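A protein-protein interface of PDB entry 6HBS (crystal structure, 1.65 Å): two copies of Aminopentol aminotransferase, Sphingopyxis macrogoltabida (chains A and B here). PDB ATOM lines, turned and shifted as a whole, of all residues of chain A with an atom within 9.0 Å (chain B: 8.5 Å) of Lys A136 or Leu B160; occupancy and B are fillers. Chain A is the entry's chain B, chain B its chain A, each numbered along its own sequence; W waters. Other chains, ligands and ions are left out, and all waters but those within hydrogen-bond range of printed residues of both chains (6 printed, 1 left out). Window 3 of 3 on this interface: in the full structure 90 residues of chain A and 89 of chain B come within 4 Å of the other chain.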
ATOM      1  N   MET A 126      -8.584 -24.221 -24.388  1.00  0.00           N
ATOM      2  CA  MET A 126      -7.480 -23.867 -23.445  1.00  0.00           C
ATOM      3  C   MET A 126      -7.983 -23.849 -21.995  1.00  0.00           C
ATOM      4  O   MET A 126      -7.444 -24.529 -21.111  1.00  0.00           O
ATOM      5  CB  MET A 126      -6.907 -22.495 -23.803  1.00  0.00           C
ATOM      6  CG  MET A 126      -5.951 -21.940 -22.746  1.00  0.00           C
ATOM      7  SD  MET A 126      -5.238 -20.352 -23.218  1.00  0.00           S
ATOM      8  CE  MET A 126      -6.559 -19.227 -22.778  1.00  0.00           C
ATOM      9  N   VAL A 127      -9.065 -23.088 -21.764  1.00  0.00           N
ATOM     10  CA  VAL A 127      -9.681 -22.972 -20.461  1.00  0.00           C
ATOM     11  C   VAL A 127     -10.240 -24.343 -20.019  1.00  0.00           C
ATOM     12  O   VAL A 127     -10.028 -24.780 -18.857  1.00  0.00           O
ATOM     13  CB  VAL A 127     -10.750 -21.859 -20.457  1.00  0.00           C
ATOM     14  CG1 VAL A 127     -11.541 -21.868 -19.165  1.00  0.00           C
ATOM     15  CG2 VAL A 127     -10.136 -20.484 -20.674  1.00  0.00           C
ATOM     16  N   ALA A 129      -9.168 -27.370 -20.980  1.00  0.00           N
ATOM     17  CA  ALA A 129      -8.069 -28.278 -20.646  1.00  0.00           C
ATOM     18  C   ALA A 129      -7.498 -27.979 -19.256  1.00  0.00           C
ATOM     19  O   ALA A 129      -7.127 -28.931 -18.547  1.00  0.00           O
ATOM     20  CB  ALA A 129      -6.987 -28.189 -21.685  1.00  0.00           C
ATOM     21  N   ARG A 130      -7.377 -26.691 -18.893  1.00  0.00           N
ATOM     22  CA  ARG A 130      -6.862 -26.327 -17.591  1.00  0.00           C
ATOM     23  C   ARG A 130      -7.838 -26.824 -16.521  1.00  0.00           C
ATOM     24  O   ARG A 130      -7.417 -27.415 -15.511  1.00  0.00           O
ATOM     25  CB  ARG A 130      -6.565 -24.826 -17.526  1.00  0.00           C
ATOM     26  CG  ARG A 130      -5.345 -24.450 -18.360  1.00  0.00           C
ATOM     27  CD  ARG A 130      -5.159 -22.971 -18.480  1.00  0.00           C
ATOM     28  NE  ARG A 130      -3.808 -22.671 -18.923  1.00  0.00           N
ATOM     29  CZ  ARG A 130      -3.438 -21.525 -19.462  1.00  0.00           C
ATOM     30  NH1 ARG A 130      -4.330 -20.556 -19.602  1.00  0.00           N
ATOM     31  NH2 ARG A 130      -2.179 -21.360 -19.864  1.00  0.00           N
ATOM     32  N   ALA A 131      -9.141 -26.625 -16.748  1.00  0.00           N
ATOM     33  CA  ALA A 131     -10.155 -27.092 -15.772  1.00  0.00           C
ATOM     34  C   ALA A 131     -10.127 -28.617 -15.638  1.00  0.00           C
ATOM     35  O   ALA A 131     -10.256 -29.150 -14.516  1.00  0.00           O
ATOM     36  CB  ALA A 131     -11.541 -26.625 -16.167  1.00  0.00           C
ATOM     37  N   THR A 133      -7.682 -30.805 -16.184  1.00  0.00           N
ATOM     38  CA  THR A 133      -6.417 -31.388 -15.666  1.00  0.00           C
ATOM     39  C   THR A 133      -6.027 -30.793 -14.314  1.00  0.00           C
ATOM     40  O   THR A 133      -5.293 -31.446 -13.546  1.00  0.00           O
ATOM     41  CB  THR A 133      -5.251 -31.163 -16.637  1.00  0.00           C
ATOM     42  OG1 THR A 133      -5.081 -29.758 -16.816  1.00  0.00           O
ATOM     43  CG2 THR A 133      -5.427 -31.860 -17.962  1.00  0.00           C
ATOM     44  N   GLY A 134      -6.439 -29.546 -14.045  1.00  0.00           N
ATOM     45  CA  GLY A 134      -5.947 -28.793 -12.917  1.00  0.00           C
ATOM     46  C   GLY A 134      -4.491 -28.362 -13.083  1.00  0.00           C
ATOM     47  O   GLY A 134      -3.829 -27.981 -12.124  1.00  0.00           O
ATOM     48  N   ARG A 135      -3.989 -28.378 -14.315  1.00  0.00           N
ATOM     49  CA  ARG A 135      -2.651 -27.985 -14.638  1.00  0.00           C
ATOM     50  C   ARG A 135      -2.679 -26.688 -15.454  1.00  0.00           C
ATOM     51  O   ARG A 135      -3.735 -26.249 -15.944  1.00  0.00           O
ATOM     52  CB  ARG A 135      -1.978 -29.126 -15.398  1.00  0.00           C
ATOM     53  CG  ARG A 135      -2.018 -30.463 -14.677  1.00  0.00           C
ATOM     54  CD  ARG A 135      -1.448 -31.532 -15.578  1.00  0.00           C
ATOM     55  NE  ARG A 135      -1.934 -32.844 -15.215  1.00  0.00           N
ATOM     56  CZ  ARG A 135      -2.035 -33.871 -16.050  1.00  0.00           C
ATOM     57  NH1 ARG A 135      -1.694 -33.750 -17.323  1.00  0.00           N
ATOM     58  NH2 ARG A 135      -2.463 -35.031 -15.594  1.00  0.00           N
ATOM     59  N   LYS A 136      -1.495 -26.095 -15.632  1.00  0.00           N
ATOM     60  CA  LYS A 136      -1.391 -24.746 -16.140  1.00  0.00           C
ATOM     61  C   LYS A 136      -0.908 -24.703 -17.587  1.00  0.00           C
ATOM     62  O   LYS A 136      -1.313 -23.777 -18.313  1.00  0.00           O
ATOM     63  CB  LYS A 136      -0.446 -23.915 -15.274  1.00  0.00           C
ATOM     64  CG  LYS A 136      -0.878 -23.775 -13.825  1.00  0.00           C
ATOM     65  CD  LYS A 136      -0.055 -22.762 -13.082  1.00  0.00           C
ATOM     66  CE  LYS A 136      -0.513 -22.629 -11.648  1.00  0.00           C
ATOM     67  NZ  LYS A 136      -0.494 -21.214 -11.213  1.00  0.00           N
ATOM     68  N   THR A 137       0.014 -25.608 -17.974  1.00  0.00           N
ATOM     69  CA  THR A 137       0.819 -25.364 -19.178  1.00  0.00           C
ATOM     70  C   THR A 137       0.109 -25.869 -20.436  1.00  0.00           C
ATOM     71  O   THR A 137      -0.341 -27.020 -20.505  1.00  0.00           O
ATOM     72  CB  THR A 137       2.246 -25.944 -19.083  1.00  0.00           C
ATOM     73  OG1 THR A 137       2.883 -25.458 -17.900  1.00  0.00           O
ATOM     74  CG2 THR A 137       3.098 -25.534 -20.255  1.00  0.00           C
ATOM     75  N   ILE A 138       0.029 -24.972 -21.421  1.00  0.00           N
ATOM     76  CA  ILE A 138      -0.482 -25.248 -22.751  1.00  0.00           C
ATOM     77  C   ILE A 138       0.720 -25.287 -23.715  1.00  0.00           C
ATOM     78  O   ILE A 138       1.432 -24.324 -23.811  1.00  0.00           O
ATOM     79  CB  ILE A 138      -1.504 -24.161 -23.166  1.00  0.00           C
ATOM     80  CG1 ILE A 138      -2.694 -24.076 -22.205  1.00  0.00           C
ATOM     81  CG2 ILE A 138      -1.947 -24.349 -24.609  1.00  0.00           C
ATOM     82  CD1 ILE A 138      -3.618 -25.259 -22.237  1.00  0.00           C
ATOM     83  N   LEU A 139       0.887 -26.390 -24.441  1.00  0.00           N
ATOM     84  CA  LEU A 139       1.940 -26.529 -25.447  1.00  0.00           C
ATOM     85  C   LEU A 139       1.400 -26.218 -26.846  1.00  0.00           C
ATOM     86  O   LEU A 139       0.453 -26.839 -27.292  1.00  0.00           O
ATOM     87  CB  LEU A 139       2.488 -27.963 -25.415  1.00  0.00           C
ATOM     88  CG  LEU A 139       3.140 -28.369 -24.103  1.00  0.00           C
ATOM     89  CD1 LEU A 139       3.639 -29.803 -24.205  1.00  0.00           C
ATOM     90  CD2 LEU A 139       4.268 -27.408 -23.754  1.00  0.00           C
ATOM     91  N   SER A 162       2.554 -11.906 -18.699  1.00  0.00           N
ATOM     92  CA  SER A 162       1.634 -12.698 -17.866  1.00  0.00           C
ATOM     93  C   SER A 162       0.471 -13.250 -18.702  1.00  0.00           C
ATOM     94  O   SER A 162      -0.142 -14.221 -18.290  1.00  0.00           O
ATOM     95  CB  SER A 162       1.097 -11.901 -16.694  1.00  0.00           C
ATOM     96  OG  SER A 162       0.514 -10.680 -17.112  1.00  0.00           O
ATOM     97  N   ASP A 163       0.204 -12.647 -19.871  1.00  0.00           N
ATOM     98  CA  ASP A 163      -0.882 -13.147 -20.769  1.00  0.00           C
ATOM     99  C   ASP A 163      -0.546 -14.551 -21.314  1.00  0.00           C
ATOM    100  O   ASP A 163      -1.453 -15.326 -21.631  1.00  0.00           O
ATOM    101  CB  ASP A 163      -1.149 -12.135 -21.883  1.00  0.00           C
ATOM    102  CG  ASP A 163      -1.780 -10.853 -21.396  1.00  0.00           C
ATOM    103  OD1 ASP A 163      -2.496 -10.899 -20.371  1.00  0.00           O
ATOM    104  OD2 ASP A 163      -1.586  -9.825 -22.061  1.00  0.00           O
ATOM    105  N   ARG A 164       0.748 -14.913 -21.373  1.00  0.00           N
ATOM    106  CA  ARG A 164       1.138 -16.189 -21.978  1.00  0.00           C
ATOM    107  C   ARG A 164       2.263 -16.878 -21.189  1.00  0.00           C
ATOM    108  O   ARG A 164       2.964 -17.749 -21.718  1.00  0.00           O
ATOM    109  CB  ARG A 164       1.540 -15.941 -23.434  1.00  0.00           C
ATOM    110  CG  ARG A 164       2.464 -14.744 -23.608  1.00  0.00           C
ATOM    111  CD  ARG A 164       2.634 -14.448 -25.068  1.00  0.00           C
ATOM    112  NE  ARG A 164       1.418 -14.052 -25.775  1.00  0.00           N
ATOM    113  CZ  ARG A 164       1.431 -13.762 -27.073  1.00  0.00           C
ATOM    114  NH1 ARG A 164       2.566 -13.908 -27.739  1.00  0.00           N
ATOM    115  NH2 ARG A 164       0.346 -13.321 -27.691  1.00  0.00           N
ATOM    116  N   VAL A 165       2.332 -16.623 -19.886  1.00  0.00           N
ATOM    117  CA  VAL A 165       3.436 -17.156 -19.093  1.00  0.00           C
ATOM    118  C   VAL A 165       3.294 -18.677 -18.946  1.00  0.00           C
ATOM    119  O   VAL A 165       4.289 -19.336 -18.691  1.00  0.00           O
ATOM    120  CB  VAL A 165       3.571 -16.462 -17.725  1.00  0.00           C
ATOM    121  CG1 VAL A 165       2.312 -16.602 -16.865  1.00  0.00           C
ATOM    122  CG2 VAL A 165       4.815 -16.973 -16.968  1.00  0.00           C
ATOM    123  N   HIS A 166       2.078 -19.233 -19.112  1.00  0.00           N
ATOM    124  CA  HIS A 166       1.856 -20.671 -19.041  1.00  0.00           C
ATOM    125  C   HIS A 166       1.516 -21.276 -20.411  1.00  0.00           C
ATOM    126  O   HIS A 166       0.854 -22.292 -20.495  1.00  0.00           O
ATOM    127  CB  HIS A 166       0.811 -21.006 -17.970  1.00  0.00           C
ATOM    128  CG  HIS A 166       1.255 -20.656 -16.589  1.00  0.00           C
ATOM    129  ND1 HIS A 166       2.311 -21.328 -15.950  1.00  0.00           N
ATOM    130  CD2 HIS A 166       0.803 -19.724 -15.719  1.00  0.00           C
ATOM    131  CE1 HIS A 166       2.474 -20.799 -14.742  1.00  0.00           C
ATOM    132  NE2 HIS A 166       1.567 -19.814 -14.582  1.00  0.00           N
ATOM    133  N   VAL A 167       2.029 -20.668 -21.476  1.00  0.00           N
ATOM    134  CA  VAL A 167       2.070 -21.238 -22.787  1.00  0.00           C
ATOM    135  C   VAL A 167       3.535 -21.583 -23.029  1.00  0.00           C
ATOM    136  O   VAL A 167       4.373 -20.727 -22.840  1.00  0.00           O
ATOM    137  CB  VAL A 167       1.551 -20.246 -23.842  1.00  0.00           C
ATOM    138  CG1 VAL A 167       1.546 -20.834 -25.239  1.00  0.00           C
ATOM    139  CG2 VAL A 167       0.160 -19.733 -23.459  1.00  0.00           C
ATOM    140  N   ALA A 168       3.822 -22.822 -23.406  1.00  0.00           N
ATOM    141  CA  ALA A 168       5.212 -23.196 -23.793  1.00  0.00           C
ATOM    142  C   ALA A 168       5.182 -23.781 -25.215  1.00  0.00           C
ATOM    143  O   ALA A 168       4.095 -24.101 -25.717  1.00  0.00           O
ATOM    144  CB  ALA A 168       5.797 -24.137 -22.758  1.00  0.00           C
ATOM    145  N   HIS A 185       7.997 -29.595 -18.323  1.00  0.00           N
ATOM    146  CA  HIS A 185       6.905 -29.131 -17.458  1.00  0.00           C
ATOM    147  C   HIS A 185       6.208 -30.362 -16.905  1.00  0.00           C
ATOM    148  O   HIS A 185       4.995 -30.509 -17.016  1.00  0.00           O
ATOM    149  CB  HIS A 185       5.921 -28.242 -18.237  1.00  0.00           C
ATOM    150  CG  HIS A 185       6.542 -27.031 -18.837  1.00  0.00           C
ATOM    151  ND1 HIS A 185       6.643 -25.856 -18.149  1.00  0.00           N
ATOM    152  CD2 HIS A 185       7.126 -26.822 -20.034  1.00  0.00           C
ATOM    153  CE1 HIS A 185       7.267 -24.964 -18.886  1.00  0.00           C
ATOM    154  NE2 HIS A 185       7.582 -25.532 -20.033  1.00  0.00           N
ATOM    155  N   GLY A 187       4.280 -33.118 -15.342  1.00  0.00           N
ATOM    156  CA  GLY A 187       3.070 -33.146 -14.550  1.00  0.00           C
ATOM    157  C   GLY A 187       2.281 -31.840 -14.592  1.00  0.00           C
ATOM    158  O   GLY A 187       1.345 -31.678 -13.825  1.00  0.00           O
ATOM    159  N   ASP A 188       2.653 -30.889 -15.458  1.00  0.00           N
ATOM    160  CA  ASP A 188       1.936 -29.617 -15.535  1.00  0.00           C
ATOM    161  C   ASP A 188       1.325 -29.374 -16.930  1.00  0.00           C
ATOM    162  O   ASP A 188       0.959 -28.257 -17.210  1.00  0.00           O
ATOM    163  CB  ASP A 188       2.817 -28.433 -15.117  1.00  0.00           C
ATOM    164  CG  ASP A 188       2.016 -27.170 -14.826  1.00  0.00           C
ATOM    165  OD1 ASP A 188       0.928 -27.252 -14.158  1.00  0.00           O
ATOM    166  OD2 ASP A 188       2.453 -26.108 -15.270  1.00  0.00           O
ATOM    167  N   ILE A 189       1.193 -30.395 -17.790  1.00  0.00           N
ATOM    168  CA  ILE A 189       0.649 -30.140 -19.135  1.00  0.00           C
ATOM    169  C   ILE A 189      -0.880 -30.322 -19.136  1.00  0.00           C
ATOM    170  O   ILE A 189      -1.401 -31.393 -18.893  1.00  0.00           O
ATOM    171  CB  ILE A 189       1.317 -31.002 -20.222  1.00  0.00           C
ATOM    172  CG1 ILE A 189       2.852 -30.876 -20.218  1.00  0.00           C
ATOM    173  CG2 ILE A 189       0.718 -30.647 -21.574  1.00  0.00           C
ATOM    174  CD1 ILE A 189       3.370 -29.467 -20.442  1.00  0.00           C
ATOM    175  N   ALA A 190      -1.588 -29.240 -19.463  1.00  0.00           N
ATOM    176  CA  ALA A 190      -3.022 -29.248 -19.577  1.00  0.00           C
ATOM    177  C   ALA A 190      -3.427 -29.734 -20.959  1.00  0.00           C
ATOM    178  O   ALA A 190      -4.356 -30.512 -21.063  1.00  0.00           O
ATOM    179  CB  ALA A 190      -3.591 -27.879 -19.295  1.00  0.00           C
ATOM    180  N   ALA A 191      -2.713 -29.266 -21.991  1.00  0.00           N
ATOM    181  CA  ALA A 191      -3.043 -29.573 -23.359  1.00  0.00           C
ATOM    182  C   ALA A 191      -1.829 -29.391 -24.283  1.00  0.00           C
ATOM    183  O   ALA A 191      -0.912 -28.617 -24.007  1.00  0.00           O
ATOM    184  CB  ALA A 191      -4.184 -28.681 -23.820  1.00  0.00           C
ATOM    185  N   PRO B 150     -10.644 -15.047 -20.455  1.00  0.00           N
ATOM    186  CA  PRO B 150      -9.917 -15.419 -19.241  1.00  0.00           C
ATOM    187  C   PRO B 150      -9.709 -14.223 -18.298  1.00  0.00           C
ATOM    188  O   PRO B 150      -9.759 -14.411 -17.070  1.00  0.00           O
ATOM    189  CB  PRO B 150      -8.602 -16.022 -19.779  1.00  0.00           C
ATOM    190  CG  PRO B 150      -9.000 -16.561 -21.160  1.00  0.00           C
ATOM    191  CD  PRO B 150     -10.001 -15.540 -21.692  1.00  0.00           C
ATOM    192  N   TRP B 151      -9.515 -13.008 -18.832  1.00  0.00           N
ATOM    193  CA  TRP B 151      -9.228 -11.841 -17.951  1.00  0.00           C
ATOM    194  C   TRP B 151     -10.452 -11.390 -17.150  1.00  0.00           C
ATOM    195  O   TRP B 151     -10.280 -10.658 -16.174  1.00  0.00           O
ATOM    196  CB  TRP B 151      -8.617 -10.638 -18.688  1.00  0.00           C
ATOM    197  CG  TRP B 151      -9.488  -9.880 -19.649  1.00  0.00           C
ATOM    198  CD1 TRP B 151      -9.731 -10.202 -20.958  1.00  0.00           C
ATOM    199  CD2 TRP B 151     -10.196  -8.645 -19.408  1.00  0.00           C
ATOM    200  NE1 TRP B 151     -10.542  -9.265 -21.539  1.00  0.00           N
ATOM    201  CE2 TRP B 151     -10.833  -8.290 -20.625  1.00  0.00           C
ATOM    202  CE3 TRP B 151     -10.342  -7.789 -18.303  1.00  0.00           C
ATOM    203  CZ2 TRP B 151     -11.608  -7.137 -20.758  1.00  0.00           C
ATOM    204  CZ3 TRP B 151     -11.092  -6.633 -18.448  1.00  0.00           C
ATOM    205  CH2 TRP B 151     -11.735  -6.320 -19.655  1.00  0.00           C
ATOM    206  N   THR B 153     -13.932 -13.344 -17.100  1.00  0.00           N
ATOM    207  CA  THR B 153     -15.077 -14.259 -16.921  1.00  0.00           C
ATOM    208  C   THR B 153     -15.417 -14.350 -15.424  1.00  0.00           C
ATOM    209  O   THR B 153     -14.510 -14.440 -14.567  1.00  0.00           O
ATOM    210  CB  THR B 153     -14.810 -15.625 -17.565  1.00  0.00           C
ATOM    211  OG1 THR B 153     -15.961 -16.456 -17.408  1.00  0.00           O
ATOM    212  CG2 THR B 153     -13.627 -16.358 -16.961  1.00  0.00           C
ATOM    213  N   THR B 156     -14.429 -18.996 -12.588  1.00  0.00           N
ATOM    214  CA  THR B 156     -13.018 -19.080 -12.832  1.00  0.00           C
ATOM    215  C   THR B 156     -12.522 -20.538 -12.920  1.00  0.00           C
ATOM    216  O   THR B 156     -11.339 -20.765 -12.806  1.00  0.00           O
ATOM    217  CB  THR B 156     -12.281 -18.205 -11.809  1.00  0.00           C
ATOM    218  OG1 THR B 156     -12.545 -18.726 -10.509  1.00  0.00           O
ATOM    219  CG2 THR B 156     -12.687 -16.748 -11.895  1.00  0.00           C
ATOM    220  N   ALA B 157     -13.389 -21.510 -13.215  1.00  0.00           N
ATOM    221  CA  ALA B 157     -12.903 -22.881 -13.589  1.00  0.00           C
ATOM    222  C   ALA B 157     -11.992 -22.781 -14.830  1.00  0.00           C
ATOM    223  O   ALA B 157     -12.374 -22.181 -15.846  1.00  0.00           O
ATOM    224  CB  ALA B 157     -14.056 -23.803 -13.843  1.00  0.00           C
ATOM    225  N   GLY B 158     -10.742 -23.249 -14.695  1.00  0.00           N
ATOM    226  CA  GLY B 158      -9.765 -23.235 -15.791  1.00  0.00           C
ATOM    227  C   GLY B 158      -9.093 -21.893 -16.002  1.00  0.00           C
ATOM    228  O   GLY B 158      -8.371 -21.717 -16.985  1.00  0.00           O
ATOM    229  N   ILE B 159      -9.321 -20.937 -15.093  1.00  0.00           N
ATOM    230  CA  ILE B 159      -8.713 -19.618 -15.177  1.00  0.00           C
ATOM    231  C   ILE B 159      -7.524 -19.547 -14.210  1.00  0.00           C
ATOM    232  O   ILE B 159      -7.643 -19.899 -13.070  1.00  0.00           O
ATOM    233  CB  ILE B 159      -9.751 -18.528 -14.875  1.00  0.00           C
ATOM    234  CG1 ILE B 159     -10.970 -18.650 -15.804  1.00  0.00           C
ATOM    235  CG2 ILE B 159      -9.132 -17.131 -14.915  1.00  0.00           C
ATOM    236  CD1 ILE B 159     -10.646 -18.598 -17.284  1.00  0.00           C
ATOM    237  N   LEU B 160      -6.377 -19.060 -14.690  1.00  0.00           N
ATOM    238  CA  LEU B 160      -5.174 -18.933 -13.868  1.00  0.00           C
ATOM    239  C   LEU B 160      -5.126 -17.521 -13.277  1.00  0.00           C
ATOM    240  O   LEU B 160      -5.555 -16.549 -13.912  1.00  0.00           O
ATOM    241  CB  LEU B 160      -3.932 -19.189 -14.732  1.00  0.00           C
ATOM    242  CG  LEU B 160      -3.916 -20.482 -15.541  1.00  0.00           C
ATOM    243  CD1 LEU B 160      -2.532 -20.725 -16.125  1.00  0.00           C
ATOM    244  CD2 LEU B 160      -4.360 -21.668 -14.695  1.00  0.00           C
ATOM    245  N   ALA B 161      -4.484 -17.407 -12.113  1.00  0.00           N
ATOM    246  CA  ALA B 161      -4.187 -16.120 -11.500  1.00  0.00           C
ATOM    247  C   ALA B 161      -3.463 -15.215 -12.498  1.00  0.00           C
ATOM    248  O   ALA B 161      -3.722 -14.015 -12.555  1.00  0.00           O
ATOM    249  CB  ALA B 161      -3.354 -16.326 -10.249  1.00  0.00           C
ATOM    250  N   SER B 162      -2.606 -15.804 -13.343  1.00  0.00           N
ATOM    251  CA  SER B 162      -1.808 -15.049 -14.290  1.00  0.00           C
ATOM    252  C   SER B 162      -2.693 -14.420 -15.390  1.00  0.00           C
ATOM    253  O   SER B 162      -2.320 -13.412 -15.985  1.00  0.00           O
ATOM    254  CB  SER B 162      -0.695 -15.896 -14.877  1.00  0.00           C
ATOM    255  OG  SER B 162      -1.201 -17.022 -15.612  1.00  0.00           O
ATOM    256  N   ASP B 163      -3.875 -14.983 -15.627  1.00  0.00           N
ATOM    257  CA  ASP B 163      -4.790 -14.438 -16.675  1.00  0.00           C
ATOM    258  C   ASP B 163      -5.302 -13.032 -16.314  1.00  0.00           C
ATOM    259  O   ASP B 163      -5.752 -12.306 -17.195  1.00  0.00           O
ATOM    260  CB  ASP B 163      -5.968 -15.392 -16.905  1.00  0.00           C
ATOM    261  CG  ASP B 163      -5.598 -16.713 -17.563  1.00  0.00           C
ATOM    262  OD1 ASP B 163      -4.637 -16.727 -18.345  1.00  0.00           O
ATOM    263  OD2 ASP B 163      -6.272 -17.739 -17.255  1.00  0.00           O
ATOM    264  N   ARG B 164      -5.310 -12.675 -15.018  1.00  0.00           N
ATOM    265  CA  ARG B 164      -5.886 -11.404 -14.568  1.00  0.00           C
ATOM    266  C   ARG B 164      -5.046 -10.755 -13.452  1.00  0.00           C
ATOM    267  O   ARG B 164      -5.565  -9.944 -12.665  1.00  0.00           O
ATOM    268  CB  ARG B 164      -7.334 -11.618 -14.108  1.00  0.00           C
ATOM    269  CG  ARG B 164      -7.496 -12.784 -13.147  1.00  0.00           C
ATOM    270  CD  ARG B 164      -8.945 -13.048 -12.904  1.00  0.00           C
ATOM    271  NE  ARG B 164      -9.719 -13.455 -14.074  1.00  0.00           N
ATOM    272  CZ  ARG B 164     -11.022 -13.685 -13.995  1.00  0.00           C
ATOM    273  NH1 ARG B 164     -11.616 -13.497 -12.828  1.00  0.00           N
ATOM    274  NH2 ARG B 164     -11.718 -14.116 -15.031  1.00  0.00           N
ATOM    275  N   VAL B 165      -3.738 -11.024 -13.437  1.00  0.00           N
ATOM    276  CA  VAL B 165      -2.866 -10.521 -12.377  1.00  0.00           C
ATOM    277  C   VAL B 165      -2.756  -8.992 -12.472  1.00  0.00           C
ATOM    278  O   VAL B 165      -2.508  -8.342 -11.472  1.00  0.00           O
ATOM    279  CB  VAL B 165      -1.476 -11.215 -12.397  1.00  0.00           C
ATOM    280  CG1 VAL B 165      -0.687 -10.940 -13.674  1.00  0.00           C
ATOM    281  CG2 VAL B 165      -0.639 -10.842 -11.164  1.00  0.00           C
HETATM  282  O   HOH W   1      -6.900 -19.906 -18.657  1.00  0.00           O
HETATM  283  O   HOH W   2      -4.457 -15.999 -21.076  1.00  0.00           O
HETATM  284  O   HOH W   3      -1.924 -16.500 -18.063  1.00  0.00           O
HETATM  285  O   HOH W   4      -2.132 -11.133 -17.580  1.00  0.00           O
HETATM  286  O   HOH W   5      -3.507 -19.720 -10.686  1.00  0.00           O
HETATM  287  O   HOH W   6      -1.134 -18.598 -12.447  1.00  0.00           O
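Ser B162 touches its own counterpart, Ser A162. Ser A162 touches Val B165, and with the chains exchanged Val A165 touches Ser B162.
O of Ser A162 sits close to O of Ser B162, 3.3 Å away.
Of the 25 printed residues of chain A, 8 touch a printed residue of chain B. Hydrophobic or aromatic side chains of chain A that line the printed part of chain B: Met A126, Val A127, Ala A131, Val A165 and His A166. Of the 13 printed residues of chain B, 7 touch a printed residue of chain A. Hydrophobic or aromatic side chains of chain B within 4 Å of the printed part of chain A: Pro B150, Ile B159, Leu B160 and Val B165. Among the printed residues, no Asp or Glu carboxylate lies within 4 Å of a Lys or Arg side-chain nitrogen of the other chain.
CE of Met A126 touches CG of Pro B150, 3.96 Å away. Ala B157 touches Val A127. Val A127 touches Gly B158. CD1 of Ile B159 touches CG1 of Val A127, 3.9 Å away. Arg A130 touches Gly B158. Arg A130 touches Leu B160. N of Ala A131 touches CA of Gly B158, 3.6 Å away. Leu B160 touches Lys A136 (CD1 to CB, 3.9 Å). Ser B162 touches Val A165 (CB to CG1, 3.7 Å). CD2 of His A166 touches CD1 of Leu B160 (3.5 Å).
The backbone carbonyl oxygen (O) of His A166 sits at hydrogen-bond distance from the backbone NH (N) of Ile A138 (3.0 Å). O of Lys A136 lies within hydrogen-bond range of NE of Arg A130 (2.8 Å). The backbone NH of Lys A136 sits at hydrogen-bond distance from the side-chain carboxylate of Asp A188 (3.1 Å). The side-chain carboxylate of Asp B163 sits at hydrogen-bond distance from the backbone NH of Leu B160 (2.9 Å). SD of Met A126 sits at hydrogen-bond distance from NH1 of Arg A130. O of His A166 is in hydrogen-bond range of NH2 of Arg A130.
Water W3 lies within hydrogen-bond range of OG of Ser B162 (2.6 Å), OD1 of Asp B163 (2.7 Å) and O of Ser A162 (2.9 Å). Water W1 lies within hydrogen-bond range of the side-chain carboxylate of Asp B163, the guanidinium group of Arg A130 and the backbone carbonyl oxygen of Gly B158. Water W4 lies within hydrogen-bond range of OG of Ser A162 (2.7 Å), O of Ser B162 (2.8 Å) and OD1 of Asp A163 (2.8 Å). Water W2 lies within hydrogen-bond range of OD1 of Asp B163 (2.8 Å) and O of Asp A163 (3.1 Å). Water W5 lies within hydrogen-bond range of the backbone NH of Ala B161 (2.9 Å) and the side-chain amino group of Lys A136 (3.4 Å). Water W6 lies within hydrogen-bond range of NZ of Lys A136 (3.0 Å) and N of Ser B162 (3.3 Å).
Printed residues of chain B within 4 Å of Arg A130: Gly B158 (3.6 Å) and Leu B160 (3.5 Å). Lys A136 touches just one residue of chain B: Leu B160. Asp A163 touches none of the printed residues of chain B. Of the printed residues of chain A, Pro B150 touches Met A126. Printed residues of chain A within 4 Å of Ile B159: Val A127 (3.9 Å). Leu B160 touches three residues of chain A. No residue of chain A comes within 4 Å of Ala B161. Arg B164 touches none of the printed residues of chain A. The nearest residue of chain A that does not touch Leu B160 is Arg A135 (4.8 Å). The nearest printed residue of chain B that does not touch Val A165 is Leu B160 (6.4 Å).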
